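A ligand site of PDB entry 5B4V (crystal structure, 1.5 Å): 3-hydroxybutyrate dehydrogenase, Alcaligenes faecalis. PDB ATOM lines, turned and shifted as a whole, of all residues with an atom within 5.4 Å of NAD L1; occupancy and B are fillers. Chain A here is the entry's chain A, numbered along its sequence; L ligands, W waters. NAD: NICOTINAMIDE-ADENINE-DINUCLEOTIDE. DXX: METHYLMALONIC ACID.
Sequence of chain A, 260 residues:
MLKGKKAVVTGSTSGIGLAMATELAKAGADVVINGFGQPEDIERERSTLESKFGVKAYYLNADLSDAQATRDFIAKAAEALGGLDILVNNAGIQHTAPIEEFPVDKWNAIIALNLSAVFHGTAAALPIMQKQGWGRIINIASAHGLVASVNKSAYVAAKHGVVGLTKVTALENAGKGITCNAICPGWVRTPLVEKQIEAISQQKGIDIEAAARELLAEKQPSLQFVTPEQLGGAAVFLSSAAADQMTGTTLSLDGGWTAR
Water W3 lies within hydrogen-bond range of an oxygen (O2B) of NAD L1 (2.6 Å) and the backbone carbonyl oxygen of Phe 36 (3.4 Å).
Water W6 bridges the backbone carbonyl oxygen (O) of Gly 92 (2.7 Å) and an oxygen (O1A) of NAD L1 (2.8 Å).
N of Leu 192 sits close to OG1 of Thr 190 (3.2 Å).
ND2 of Asn 90 is in hydrogen-bond range of O of Gly 11, at 2.9 Å.
The backbone carbonyl oxygen (O) of Phe 36 is in hydrogen-bond range of the side-chain hydroxyl (OG1) of Thr 13, 2.6 Å away.
The backbone carbonyl oxygen (O) of Asn 34 lies within hydrogen-bond range of the backbone NH (N) of Thr 13 (3.4 Å).
The side-chain amino group of Lys 159 lies within hydrogen-bond range of the backbone carbonyl oxygen of Ile 140, 2.9 Å away.
The side-chain carboxylate (OD2) of Asp 63 is in hydrogen-bond range of the side-chain hydroxyl (OG) of Ser 65, 2.7 Å away.
The backbone NH of Gly 11 is in hydrogen-bond range of the side-chain amide oxygen of Asn 34 (3.0 Å).
The backbone carbonyl oxygen (O) of Ala 62 lies within hydrogen-bond range of the side-chain amide nitrogen (ND2) of Asn 34, at 3.4 Å.
OG1 of Thr 190 sits at hydrogen-bond distance from O1N of NAD L1 (2.6 Å).
OH of Tyr 155 is in hydrogen-bond range of O2D of NAD L1 (2.6 Å).
The backbone carbonyl oxygen (O) of Asn 90 lies within hydrogen-bond range of an oxygen (O3D) of NAD L1, at 2.7 Å.
N of Ser 14 sits at hydrogen-bond distance from O3B of NAD L1 (3.5 Å).
The side-chain hydroxyl (OG) of Ser 14 is in hydrogen-bond range of an oxygen (O2A) of NAD L1 (2.7 Å).
N of Thr 13 lies within hydrogen-bond range of O3B of NAD L1 (3.3 Å).
The side-chain hydroxyl (OG1) of Thr 13 lies within hydrogen-bond range of an oxygen (O3B) of NAD L1 (2.8 Å).
O7N of NAD L1 is in hydrogen-bond range of N of Val 188, 2.8 Å away.
O of Val 188 lies within hydrogen-bond range of N7N of NAD L1 (3.1 Å).
O2N of NAD L1 is in hydrogen-bond range of N of Ile 16 (2.8 Å).
An oxygen (O3D) of NAD L1 lies within hydrogen-bond range of the side-chain amino group (NZ) of Lys 159, at 2.9 Å.
The side-chain carboxylate (OD2) of Asp 63 is in hydrogen-bond range of a nitrogen (N6A) of NAD L1.
The backbone NH (N) of Phe 36 lies within hydrogen-bond range of an oxygen (O2B) of NAD L1, 2.9 Å away.
N of Leu 64 lies within hydrogen-bond range of N1A of NAD L1 (3.0 Å).
O3B of NAD L1 sits close to O of Gly 11, at 3.2 Å.
An oxygen (O2) of DXX L2 lies within hydrogen-bond range of the side-chain hydroxyl (OH) of Tyr 155, at 2.4 Å.
An oxygen (O) of DXX L2 lies within hydrogen-bond range of the side-chain hydroxyl of Ser 142 (2.5 Å).
O of Ala 62 lies close to N1A of NAD L1 (3.5 Å).
An oxygen (O7N) of NAD L1 sits close to the backbone carbonyl oxygen (O) of Gly 186 (3.4 Å).
Merely in contact with NAD L1: Ala 141, Val 193, Pro 185, Pro 191, Leu 113, Gly 15, Ser 142, Trp 187, Ile 140, Leu 192, Gly 92, Asn 34, Ser 12, Ala 91 and Gly 35.
Hydrophobic or aromatic side chains that line NAD L1: Ile 16, Phe 36, Leu 64, Ala 91, Leu 113, Ile 140, Tyr 155, Pro 185, Val 188, Pro 191, Leu 192 and Val 193.
29 residues have an atom within 4 Å of NAD L1: Gly 11, Ser 12, Thr 13, Ser 14, Gly 15, Ile 16, Asn 34, Gly 35, Phe 36, Ala 62, Asp 63, Leu 64, Asn 90, Ala 91, Gly 92, Leu 113, Ile 140, Ala 141, Ser 142, Tyr 155, Lys 159, Pro 185, Gly 186, Trp 187, Val 188, Thr 190, Pro 191, Leu 192 and Val 193.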
ATOM      1  N   GLY A  11      27.694  26.332  14.716  1.00  0.00           N
ATOM      2  CA  GLY A  11      28.796  25.392  14.888  1.00  0.00           C
ATOM      3  C   GLY A  11      29.205  24.725  13.580  1.00  0.00           C
ATOM      4  O   GLY A  11      29.356  23.495  13.528  1.00  0.00           O
ATOM      5  N   SER A  12      29.424  25.531  12.545  1.00  0.00           N
ATOM      6  CA  SER A  12      29.716  25.035  11.189  1.00  0.00           C
ATOM      7  C   SER A  12      31.162  25.315  10.771  1.00  0.00           C
ATOM      8  O   SER A  12      31.511  25.178   9.603  1.00  0.00           O
ATOM      9  CB  SER A  12      28.727  25.627  10.193  1.00  0.00           C
ATOM     10  OG  SER A  12      28.544  27.033  10.420  1.00  0.00           O
ATOM     11  N   THR A  13      32.036  25.469  11.760  1.00  0.00           N
ATOM     12  CA  THR A  13      33.481  25.595  11.500  1.00  0.00           C
ATOM     13  C   THR A  13      34.229  24.253  11.635  1.00  0.00           C
ATOM     14  O   THR A  13      35.429  24.173  11.376  1.00  0.00           O
ATOM     15  CB  THR A  13      34.128  26.632  12.447  1.00  0.00           C
ATOM     16  OG1 THR A  13      33.834  26.283  13.810  1.00  0.00           O
ATOM     17  CG2 THR A  13      33.612  28.031  12.155  1.00  0.00           C
ATOM     18  N   SER A  14      33.504  23.174  11.951  1.00  0.00           N
ATOM     19  CA  SER A  14      34.107  21.857  12.189  1.00  0.00           C
ATOM     20  C   SER A  14      33.018  20.826  11.909  1.00  0.00           C
ATOM     21  O   SER A  14      31.831  21.105  12.053  1.00  0.00           O
ATOM     22  CB  SER A  14      34.569  21.737  13.657  1.00  0.00           C
ATOM     23  OG  SER A  14      35.111  20.456  13.959  1.00  0.00           O
ATOM     24  N   GLY A  15      33.432  19.595  11.634  1.00  0.00           N
ATOM     25  CA  GLY A  15      32.571  18.437  11.881  1.00  0.00           C
ATOM     26  C   GLY A  15      31.289  18.453  11.079  1.00  0.00           C
ATOM     27  O   GLY A  15      31.265  18.755   9.873  1.00  0.00           O
ATOM     28  N   ILE A  16      30.223  18.022  11.720  1.00  0.00           N
ATOM     29  CA  ILE A  16      28.969  17.856  11.052  1.00  0.00           C
ATOM     30  C   ILE A  16      28.445  19.187  10.485  1.00  0.00           C
ATOM     31  O   ILE A  16      27.912  19.241   9.370  1.00  0.00           O
ATOM     32  CB  ILE A  16      27.944  17.236  12.023  1.00  0.00           C
ATOM     33  CG1 ILE A  16      28.345  15.794  12.374  1.00  0.00           C
ATOM     34  CG2 ILE A  16      26.526  17.304  11.454  1.00  0.00           C
ATOM     35  CD1 ILE A  16      27.626  15.233  13.570  1.00  0.00           C
ATOM     36  N   GLY A  17      28.564  20.249  11.274  1.00  0.00           N
ATOM     37  CA  GLY A  17      28.090  21.549  10.837  1.00  0.00           C
ATOM     38  C   GLY A  17      28.780  22.082   9.607  1.00  0.00           C
ATOM     39  O   GLY A  17      28.148  22.705   8.740  1.00  0.00           O
ATOM     40  N   ASN A  34      29.350  29.808  11.511  1.00  0.00           N
ATOM     41  CA  ASN A  34      29.440  30.192  12.910  1.00  0.00           C
ATOM     42  C   ASN A  34      30.288  29.167  13.636  1.00  0.00           C
ATOM     43  O   ASN A  34      30.335  28.012  13.226  1.00  0.00           O
ATOM     44  CB  ASN A  34      28.018  30.241  13.510  1.00  0.00           C
ATOM     45  CG  ASN A  34      28.033  30.224  15.020  1.00  0.00           C
ATOM     46  OD1 ASN A  34      27.798  29.181  15.635  1.00  0.00           O
ATOM     47  ND2 ASN A  34      28.229  31.383  15.633  1.00  0.00           N
ATOM     48  N   GLY A  35      30.984  29.591  14.693  1.00  0.00           N
ATOM     49  CA  GLY A  35      31.765  28.676  15.490  1.00  0.00           C
ATOM     50  C   GLY A  35      33.161  29.188  15.767  1.00  0.00           C
ATOM     51  O   GLY A  35      33.584  30.223  15.264  1.00  0.00           O
ATOM     52  N   PHE A  36      33.886  28.378  16.513  1.00  0.00           N
ATOM     53  CA  PHE A  36      35.251  28.704  16.896  1.00  0.00           C
ATOM     54  C   PHE A  36      36.235  28.062  15.942  1.00  0.00           C
ATOM     55  O   PHE A  36      35.907  27.152  15.170  1.00  0.00           O
ATOM     56  CB  PHE A  36      35.499  28.223  18.322  1.00  0.00           C
ATOM     57  CG  PHE A  36      34.563  28.820  19.339  1.00  0.00           C
ATOM     58  CD1 PHE A  36      33.927  28.012  20.275  1.00  0.00           C
ATOM     59  CD2 PHE A  36      34.187  30.147  19.261  1.00  0.00           C
ATOM     60  CE1 PHE A  36      33.129  28.569  21.251  1.00  0.00           C
ATOM     61  CE2 PHE A  36      33.261  30.676  20.134  1.00  0.00           C
ATOM     62  CZ  PHE A  36      32.798  29.905  21.183  1.00  0.00           C
ATOM     63  N   GLY A  37      37.489  28.493  16.037  1.00  0.00           N
ATOM     64  CA  GLY A  37      38.557  27.889  15.262  1.00  0.00           C
ATOM     65  C   GLY A  37      39.607  28.916  14.858  1.00  0.00           C
ATOM     66  O   GLY A  37      39.535  30.067  15.252  1.00  0.00           O
ATOM     67  N   ALA A  62      29.713  34.065  17.303  1.00  0.00           N
ATOM     68  CA  ALA A  62      28.849  34.207  18.460  1.00  0.00           C
ATOM     69  C   ALA A  62      29.011  32.997  19.360  1.00  0.00           C
ATOM     70  O   ALA A  62      29.070  31.862  18.874  1.00  0.00           O
ATOM     71  CB  ALA A  62      27.397  34.340  18.019  1.00  0.00           C
ATOM     72  N   ASP A  63      29.240  33.244  20.639  1.00  0.00           N
ATOM     73  CA  ASP A  63      29.230  32.197  21.642  1.00  0.00           C
ATOM     74  C   ASP A  63      27.796  31.910  22.061  1.00  0.00           C
ATOM     75  O   ASP A  63      27.134  32.730  22.694  1.00  0.00           O
ATOM     76  CB  ASP A  63      30.065  32.625  22.860  1.00  0.00           C
ATOM     77  CG  ASP A  63      30.129  31.564  23.936  1.00  0.00           C
ATOM     78  OD1 ASP A  63      30.985  31.670  24.841  1.00  0.00           O
ATOM     79  OD2 ASP A  63      29.342  30.602  23.891  1.00  0.00           O
ATOM     80  N   LEU A  64      27.259  30.806  21.547  1.00  0.00           N
ATOM     81  CA  LEU A  64      25.831  30.551  21.651  1.00  0.00           C
ATOM     82  C   LEU A  64      25.440  29.979  23.017  1.00  0.00           C
ATOM     83  O   LEU A  64      24.263  29.758  23.258  1.00  0.00           O
ATOM     84  CB  LEU A  64      25.400  29.610  20.533  1.00  0.00           C
ATOM     85  CG  LEU A  64      25.676  30.145  19.118  1.00  0.00           C
ATOM     86  CD1 LEU A  64      25.314  29.109  18.066  1.00  0.00           C
ATOM     87  CD2 LEU A  64      24.976  31.470  18.844  1.00  0.00           C
ATOM     88  N   SER A  65      26.383  29.916  23.945  1.00  0.00           N
ATOM     89  CA  SER A  65      26.038  29.635  25.323  1.00  0.00           C
ATOM     90  C   SER A  65      25.406  30.840  25.997  1.00  0.00           C
ATOM     91  O   SER A  65      24.790  30.708  27.044  1.00  0.00           O
ATOM     92  CB  SER A  65      27.259  29.161  26.113  1.00  0.00           C
ATOM     93  OG  SER A  65      28.192  30.215  26.290  1.00  0.00           O
ATOM     94  N   ASN A  90      23.070  23.249  15.292  1.00  0.00           N
ATOM     95  CA  ASN A  90      24.041  22.152  15.300  1.00  0.00           C
ATOM     96  C   ASN A  90      25.111  22.224  16.392  1.00  0.00           C
ATOM     97  O   ASN A  90      25.577  21.184  16.861  1.00  0.00           O
ATOM     98  CB  ASN A  90      24.678  22.027  13.906  1.00  0.00           C
ATOM     99  CG  ASN A  90      25.914  21.173  13.916  1.00  0.00           C
ATOM    100  OD1 ASN A  90      25.837  19.937  13.820  1.00  0.00           O
ATOM    101  ND2 ASN A  90      27.081  21.816  14.049  1.00  0.00           N
ATOM    102  N   ALA A  91      25.502  23.426  16.816  1.00  0.00           N
ATOM    103  CA  ALA A  91      26.624  23.569  17.739  1.00  0.00           C
ATOM    104  C   ALA A  91      26.371  22.746  18.992  1.00  0.00           C
ATOM    105  O   ALA A  91      25.270  22.746  19.551  1.00  0.00           O
ATOM    106  CB  ALA A  91      26.851  25.027  18.097  1.00  0.00           C
ATOM    107  N   GLY A  92      27.401  22.039  19.463  1.00  0.00           N
ATOM    108  CA  GLY A  92      27.266  21.240  20.668  1.00  0.00           C
ATOM    109  C   GLY A  92      28.617  20.835  21.187  1.00  0.00           C
ATOM    110  O   GLY A  92      29.593  20.821  20.420  1.00  0.00           O
ATOM    111  N   ILE A  93      28.657  20.491  22.461  1.00  0.00           N
ATOM    112  CA  ILE A  93      29.839  19.967  23.121  1.00  0.00           C
ATOM    113  C   ILE A  93      29.476  18.713  23.919  1.00  0.00           C
ATOM    114  O   ILE A  93      28.303  18.435  24.197  1.00  0.00           O
ATOM    115  CB  ILE A  93      30.470  21.018  24.059  1.00  0.00           C
ATOM    116  CG1 ILE A  93      29.431  21.569  25.028  1.00  0.00           C
ATOM    117  CG2 ILE A  93      31.080  22.172  23.249  1.00  0.00           C
ATOM    118  CD1 ILE A  93      30.027  22.460  26.096  1.00  0.00           C
ATOM    119  N   LEU A 113      24.504  25.348  25.748  1.00  0.00           N
ATOM    120  CA  LEU A 113      24.762  25.270  24.314  1.00  0.00           C
ATOM    121  C   LEU A 113      23.861  24.247  23.651  1.00  0.00           C
ATOM    122  O   LEU A 113      23.238  24.529  22.617  1.00  0.00           O
ATOM    123  CB  LEU A 113      26.223  24.924  24.015  1.00  0.00           C
ATOM    124  CG  LEU A 113      26.563  24.891  22.528  1.00  0.00           C
ATOM    125  CD1 LEU A 113      26.316  26.239  21.859  1.00  0.00           C
ATOM    126  CD2 LEU A 113      28.004  24.452  22.362  1.00  0.00           C
ATOM    127  N   ASN A 114      23.843  23.041  24.192  1.00  0.00           N
ATOM    128  CA  ASN A 114      23.206  21.925  23.487  1.00  0.00           C
ATOM    129  C   ASN A 114      21.677  21.985  23.566  1.00  0.00           C
ATOM    130  O   ASN A 114      21.001  21.334  22.765  1.00  0.00           O
ATOM    131  CB  ASN A 114      23.656  20.574  24.024  1.00  0.00           C
ATOM    132  CG  ASN A 114      25.122  20.275  23.774  1.00  0.00           C
ATOM    133  OD1 ASN A 114      25.947  21.155  23.576  1.00  0.00           O
ATOM    134  ND2 ASN A 114      25.479  19.005  23.881  1.00  0.00           N
ATOM    135  N   ILE A 140      20.097  19.297  15.404  1.00  0.00           N
ATOM    136  CA  ILE A 140      20.978  18.142  15.472  1.00  0.00           C
ATOM    137  C   ILE A 140      20.997  17.634  16.895  1.00  0.00           C
ATOM    138  O   ILE A 140      21.587  18.266  17.771  1.00  0.00           O
ATOM    139  CB  ILE A 140      22.400  18.474  15.026  1.00  0.00           C
ATOM    140  CG1 ILE A 140      22.389  19.177  13.673  1.00  0.00           C
ATOM    141  CG2 ILE A 140      23.220  17.183  14.936  1.00  0.00           C
ATOM    142  CD1 ILE A 140      21.620  18.478  12.577  1.00  0.00           C
ATOM    143  N   ALA A 141      20.203  16.605  17.136  1.00  0.00           N
ATOM    144  CA  ALA A 141      20.165  15.960  18.424  1.00  0.00           C
ATOM    145  C   ALA A 141      21.206  14.861  18.461  1.00  0.00           C
ATOM    146  O   ALA A 141      22.385  15.166  18.272  1.00  0.00           O
ATOM    147  CB  ALA A 141      18.764  15.470  18.745  1.00  0.00           C
ATOM    148  N   SER A 142      20.796  13.602  18.635  1.00  0.00           N
ATOM    149  CA  SER A 142      21.722  12.466  18.764  1.00  0.00           C
ATOM    150  C   SER A 142      20.867  11.213  18.972  1.00  0.00           C
ATOM    151  O   SER A 142      19.714  11.297  19.418  1.00  0.00           O
ATOM    152  CB  SER A 142      22.636  12.646  19.976  1.00  0.00           C
ATOM    153  OG  SER A 142      23.465  11.517  20.194  1.00  0.00           O
ATOM    154  N   ALA A 143      21.468  10.050  18.786  1.00  0.00           N
ATOM    155  CA  ALA A 143      20.928   8.833  19.378  1.00  0.00           C
ATOM    156  C   ALA A 143      20.668   9.018  20.872  1.00  0.00           C
ATOM    157  O   ALA A 143      19.706   8.478  21.423  1.00  0.00           O
ATOM    158  CB  ALA A 143      21.879   7.669  19.147  1.00  0.00           C
ATOM    159  N   TYR A 155      24.677  15.569  28.613  1.00  0.00           N
ATOM    160  CA  TYR A 155      24.502  15.511  27.174  1.00  0.00           C
ATOM    161  C   TYR A 155      23.196  14.770  26.816  1.00  0.00           C
ATOM    162  O   TYR A 155      22.427  15.232  25.969  1.00  0.00           O
ATOM    163  CB  TYR A 155      25.705  14.786  26.548  1.00  0.00           C
ATOM    164  CG  TYR A 155      25.705  14.759  25.035  1.00  0.00           C
ATOM    165  CD1 TYR A 155      25.159  13.689  24.342  1.00  0.00           C
ATOM    166  CD2 TYR A 155      26.266  15.801  24.303  1.00  0.00           C
ATOM    167  CE1 TYR A 155      25.189  13.654  22.960  1.00  0.00           C
ATOM    168  CE2 TYR A 155      26.393  15.723  22.930  1.00  0.00           C
ATOM    169  CZ  TYR A 155      25.811  14.668  22.270  1.00  0.00           C
ATOM    170  OH  TYR A 155      25.873  14.604  20.888  1.00  0.00           O
ATOM    171  N   LYS A 159      20.052  16.476  24.956  1.00  0.00           N
ATOM    172  CA  LYS A 159      19.602  15.977  23.670  1.00  0.00           C
ATOM    173  C   LYS A 159      18.173  15.443  23.718  1.00  0.00           C
ATOM    174  O   LYS A 159      17.424  15.636  22.769  1.00  0.00           O
ATOM    175  CB  LYS A 159      20.568  14.918  23.120  1.00  0.00           C
ATOM    176  CG  LYS A 159      21.962  15.450  22.796  1.00  0.00           C
ATOM    177  CD  LYS A 159      21.922  16.508  21.702  1.00  0.00           C
ATOM    178  CE  LYS A 159      23.312  16.754  21.092  1.00  0.00           C
ATOM    179  NZ  LYS A 159      23.301  17.781  20.029  1.00  0.00           N
ATOM    180  N   PRO A 185      22.077  11.557  14.956  1.00  0.00           N
ATOM    181  CA  PRO A 185      23.182  10.701  14.519  1.00  0.00           C
ATOM    182  C   PRO A 185      23.668   9.742  15.591  1.00  0.00           C
ATOM    183  O   PRO A 185      23.628  10.047  16.789  1.00  0.00           O
ATOM    184  CB  PRO A 185      24.293  11.700  14.156  1.00  0.00           C
ATOM    185  CG  PRO A 185      23.648  13.042  14.132  1.00  0.00           C
ATOM    186  CD  PRO A 185      22.476  12.965  15.063  1.00  0.00           C
ATOM    187  N   GLY A 186      24.147   8.588  15.144  1.00  0.00           N
ATOM    188  CA  GLY A 186      25.094   7.779  15.905  1.00  0.00           C
ATOM    189  C   GLY A 186      26.502   8.338  15.805  1.00  0.00           C
ATOM    190  O   GLY A 186      26.698   9.526  15.555  1.00  0.00           O
ATOM    191  N   TRP A 187      27.499   7.474  15.986  1.00  0.00           N
ATOM    192  CA  TRP A 187      28.882   7.917  15.947  1.00  0.00           C
ATOM    193  C   TRP A 187      29.256   8.461  14.582  1.00  0.00           C
ATOM    194  O   TRP A 187      29.072   7.790  13.555  1.00  0.00           O
ATOM    195  CB  TRP A 187      29.843   6.766  16.268  1.00  0.00           C
ATOM    196  CG  TRP A 187      29.737   6.176  17.640  1.00  0.00           C
ATOM    197  CD1 TRP A 187      29.478   4.876  17.933  1.00  0.00           C
ATOM    198  CD2 TRP A 187      30.094   6.792  18.889  1.00  0.00           C
ATOM    199  NE1 TRP A 187      29.668   4.630  19.272  1.00  0.00           N
ATOM    200  CE2 TRP A 187      29.971   5.818  19.890  1.00  0.00           C
ATOM    201  CE3 TRP A 187      30.579   8.056  19.239  1.00  0.00           C
ATOM    202  CZ2 TRP A 187      30.303   6.069  21.225  1.00  0.00           C
ATOM    203  CZ3 TRP A 187      30.935   8.289  20.560  1.00  0.00           C
ATOM    204  CH2 TRP A 187      30.746   7.311  21.539  1.00  0.00           C
ATOM    205  N   VAL A 188      29.895   9.632  14.614  1.00  0.00           N
ATOM    206  CA  VAL A 188      30.442  10.341  13.453  1.00  0.00           C
ATOM    207  C   VAL A 188      31.849  10.757  13.857  1.00  0.00           C
ATOM    208  O   VAL A 188      32.048  11.284  14.957  1.00  0.00           O
ATOM    209  CB  VAL A 188      29.618  11.605  13.158  1.00  0.00           C
ATOM    210  CG1 VAL A 188      30.131  12.311  11.916  1.00  0.00           C
ATOM    211  CG2 VAL A 188      28.141  11.273  13.003  1.00  0.00           C
ATOM    212  N   ARG A 189      32.845  10.444  13.049  1.00  0.00           N
ATOM    213  CA  ARG A 189      34.212  10.643  13.483  1.00  0.00           C
ATOM    214  C   ARG A 189      34.670  12.085  13.316  1.00  0.00           C
ATOM    215  O   ARG A 189      35.405  12.415  12.389  1.00  0.00           O
ATOM    216  CB  ARG A 189      35.149   9.698  12.760  1.00  0.00           C
ATOM    217  CG  ARG A 189      36.465   9.546  13.503  1.00  0.00           C
ATOM    218  CD  ARG A 189      37.291   8.398  13.003  1.00  0.00           C
ATOM    219  NE  ARG A 189      38.461   8.242  13.855  1.00  0.00           N
ATOM    220  CZ  ARG A 189      39.269   7.184  13.832  1.00  0.00           C
ATOM    221  NH1 ARG A 189      39.139   6.294  12.864  1.00  0.00           N
ATOM    222  NH2 ARG A 189      40.359   7.196  14.583  1.00  0.00           N
ATOM    223  N   THR A 190      34.260  12.921  14.268  1.00  0.00           N
ATOM    224  CA  THR A 190      34.642  14.320  14.335  1.00  0.00           C
ATOM    225  C   THR A 190      35.596  14.483  15.540  1.00  0.00           C
ATOM    226  O   THR A 190      35.720  13.559  16.354  1.00  0.00           O
ATOM    227  CB  THR A 190      33.401  15.203  14.591  1.00  0.00           C
ATOM    228  OG1 THR A 190      32.895  14.917  15.901  1.00  0.00           O
ATOM    229  CG2 THR A 190      32.316  14.945  13.539  1.00  0.00           C
ATOM    230  N   PRO A 191      36.063  15.714  15.802  1.00  0.00           N
ATOM    231  CA  PRO A 191      36.883  15.900  17.004  1.00  0.00           C
ATOM    232  C   PRO A 191      36.156  15.590  18.322  1.00  0.00           C
ATOM    233  O   PRO A 191      36.780  15.156  19.289  1.00  0.00           O
ATOM    234  CB  PRO A 191      37.277  17.381  16.947  1.00  0.00           C
ATOM    235  CG  PRO A 191      37.191  17.739  15.499  1.00  0.00           C
ATOM    236  CD  PRO A 191      36.093  16.889  14.919  1.00  0.00           C
ATOM    237  N   LEU A 192      34.835  15.722  18.312  1.00  0.00           N
ATOM    238  CA  LEU A 192      34.055  15.437  19.513  1.00  0.00           C
ATOM    239  C   LEU A 192      34.166  13.961  19.917  1.00  0.00           C
ATOM    240  O   LEU A 192      34.108  13.613  21.104  1.00  0.00           O
ATOM    241  CB  LEU A 192      32.588  15.807  19.257  1.00  0.00           C
ATOM    242  CG  LEU A 192      31.576  15.633  20.385  1.00  0.00           C
ATOM    243  CD1 LEU A 192      30.472  16.651  20.207  1.00  0.00           C
ATOM    244  CD2 LEU A 192      30.995  14.219  20.406  1.00  0.00           C
ATOM    245  N   VAL A 193      34.285  13.095  18.910  1.00  0.00           N
ATOM    246  CA  VAL A 193      34.362  11.655  19.082  1.00  0.00           C
ATOM    247  C   VAL A 193      35.814  11.183  19.165  1.00  0.00           C
ATOM    248  O   VAL A 193      36.124  10.231  19.865  1.00  0.00           O
ATOM    249  CB  VAL A 193      33.613  10.963  17.925  1.00  0.00           C
ATOM    250  CG1 VAL A 193      33.993   9.490  17.798  1.00  0.00           C
ATOM    251  CG2 VAL A 193      32.115  11.115  18.131  1.00  0.00           C
HETATM  252  PA  NAD L   1      32.645  19.328  16.526  1.00  0.00           P
HETATM  253  O1A NAD L   1      33.327  19.537  17.824  1.00  0.00           O
HETATM  254  O2A NAD L   1      33.401  18.878  15.308  1.00  0.00           O
HETATM  255  O5B NAD L   1      31.952  20.695  16.113  1.00  0.00           O
HETATM  256  C5B NAD L   1      31.334  21.531  17.085  1.00  0.00           C
HETATM  257  C4B NAD L   1      31.029  22.850  16.412  1.00  0.00           C
HETATM  258  O4B NAD L   1      30.354  23.695  17.353  1.00  0.00           O
HETATM  259  C3B NAD L   1      32.328  23.599  16.077  1.00  0.00           C
HETATM  260  O3B NAD L   1      32.092  24.403  14.906  1.00  0.00           O
HETATM  261  C2B NAD L   1      32.554  24.452  17.312  1.00  0.00           C
HETATM  262  O2B NAD L   1      33.415  25.586  17.088  1.00  0.00           O
HETATM  263  C1B NAD L   1      31.126  24.879  17.587  1.00  0.00           C
HETATM  264  N9A NAD L   1      30.944  25.393  18.937  1.00  0.00           N
HETATM  265  C8A NAD L   1      31.310  24.810  20.099  1.00  0.00           C
HETATM  266  N7A NAD L   1      31.011  25.614  21.145  1.00  0.00           N
HETATM  267  C5A NAD L   1      30.308  26.667  20.653  1.00  0.00           C
HETATM  268  C6A NAD L   1      29.683  27.873  21.196  1.00  0.00           C
HETATM  269  N6A NAD L   1      29.660  28.092  22.526  1.00  0.00           N
HETATM  270  N1A NAD L   1      29.092  28.703  20.320  1.00  0.00           N
HETATM  271  C2A NAD L   1      29.079  28.492  18.989  1.00  0.00           C
HETATM  272  N3A NAD L   1      29.697  27.440  18.418  1.00  0.00           N
HETATM  273  C4A NAD L   1      30.262  26.505  19.212  1.00  0.00           C
HETATM  274  O3  NAD L   1      31.428  18.315  16.882  1.00  0.00           O
HETATM  275  PN  NAD L   1      30.385  17.534  15.961  1.00  0.00           P
HETATM  276  O1N NAD L   1      30.619  16.092  16.267  1.00  0.00           O
HETATM  277  O2N NAD L   1      30.432  18.014  14.550  1.00  0.00           O
HETATM  278  O5D NAD L   1      28.999  17.983  16.639  1.00  0.00           O
HETATM  279  C5D NAD L   1      27.995  18.741  15.967  1.00  0.00           C
HETATM  280  C4D NAD L   1      26.660  18.351  16.584  1.00  0.00           C
HETATM  281  O4D NAD L   1      26.444  16.945  16.333  1.00  0.00           O
HETATM  282  C3D NAD L   1      26.617  18.532  18.106  1.00  0.00           C
HETATM  283  O3D NAD L   1      25.327  19.058  18.481  1.00  0.00           O
HETATM  284  C2D NAD L   1      26.739  17.114  18.650  1.00  0.00           C
HETATM  285  O2D NAD L   1      26.101  17.003  19.924  1.00  0.00           O
HETATM  286  C1D NAD L   1      26.018  16.341  17.552  1.00  0.00           C
HETATM  287  N1N NAD L   1      26.293  14.917  17.510  1.00  0.00           N
HETATM  288  C2N NAD L   1      27.540  14.463  17.232  1.00  0.00           C
HETATM  289  C3N NAD L   1      27.758  13.091  17.097  1.00  0.00           C
HETATM  290  C7N NAD L   1      29.105  12.515  16.761  1.00  0.00           C
HETATM  291  O7N NAD L   1      29.258  11.304  16.793  1.00  0.00           O
HETATM  292  N7N NAD L   1      30.090  13.317  16.354  1.00  0.00           N
HETATM  293  C4N NAD L   1      26.709  12.197  17.312  1.00  0.00           C
HETATM  294  C5N NAD L   1      25.446  12.699  17.610  1.00  0.00           C
HETATM  295  C6N NAD L   1      25.252  14.076  17.637  1.00  0.00           C
HETATM  296  C1  DXX L   2      28.563  10.560  21.894  1.00  0.00           C
HETATM  297  O1  DXX L   2      29.413  11.367  22.326  1.00  0.00           O
HETATM  298  OXT DXX L   2      27.978   9.743  22.624  1.00  0.00           O
HETATM  299  CA  DXX L   2      28.102  10.691  20.477  1.00  0.00           C
HETATM  300  CB  DXX L   2      27.557   9.371  19.933  1.00  0.00           C
HETATM  301  C   DXX L   2      27.060  11.745  20.432  1.00  0.00           C
HETATM  302  O   DXX L   2      25.896  11.464  20.828  1.00  0.00           O
HETATM  303  O2  DXX L   2      27.469  12.900  20.245  1.00  0.00           O
HETATM  304  O   HOH W   1      30.546  26.590  24.886  1.00  0.00           O
HETATM  305  O   HOH W   2      32.649  25.444  23.447  1.00  0.00           O
HETATM  306  O   HOH W   3      35.798  24.546  17.347  1.00  0.00           O
HETATM  307  O   HOH W   4      29.710  20.551  13.888  1.00  0.00           O
HETATM  308  O   HOH W   5      33.628  22.507  20.304  1.00  0.00           O
HETATM  309  O   HOH W   6      32.234  20.070  20.329  1.00  0.00           O
HETATM  310  O   HOH W   7      35.285  21.779  17.769  1.00  0.00           O
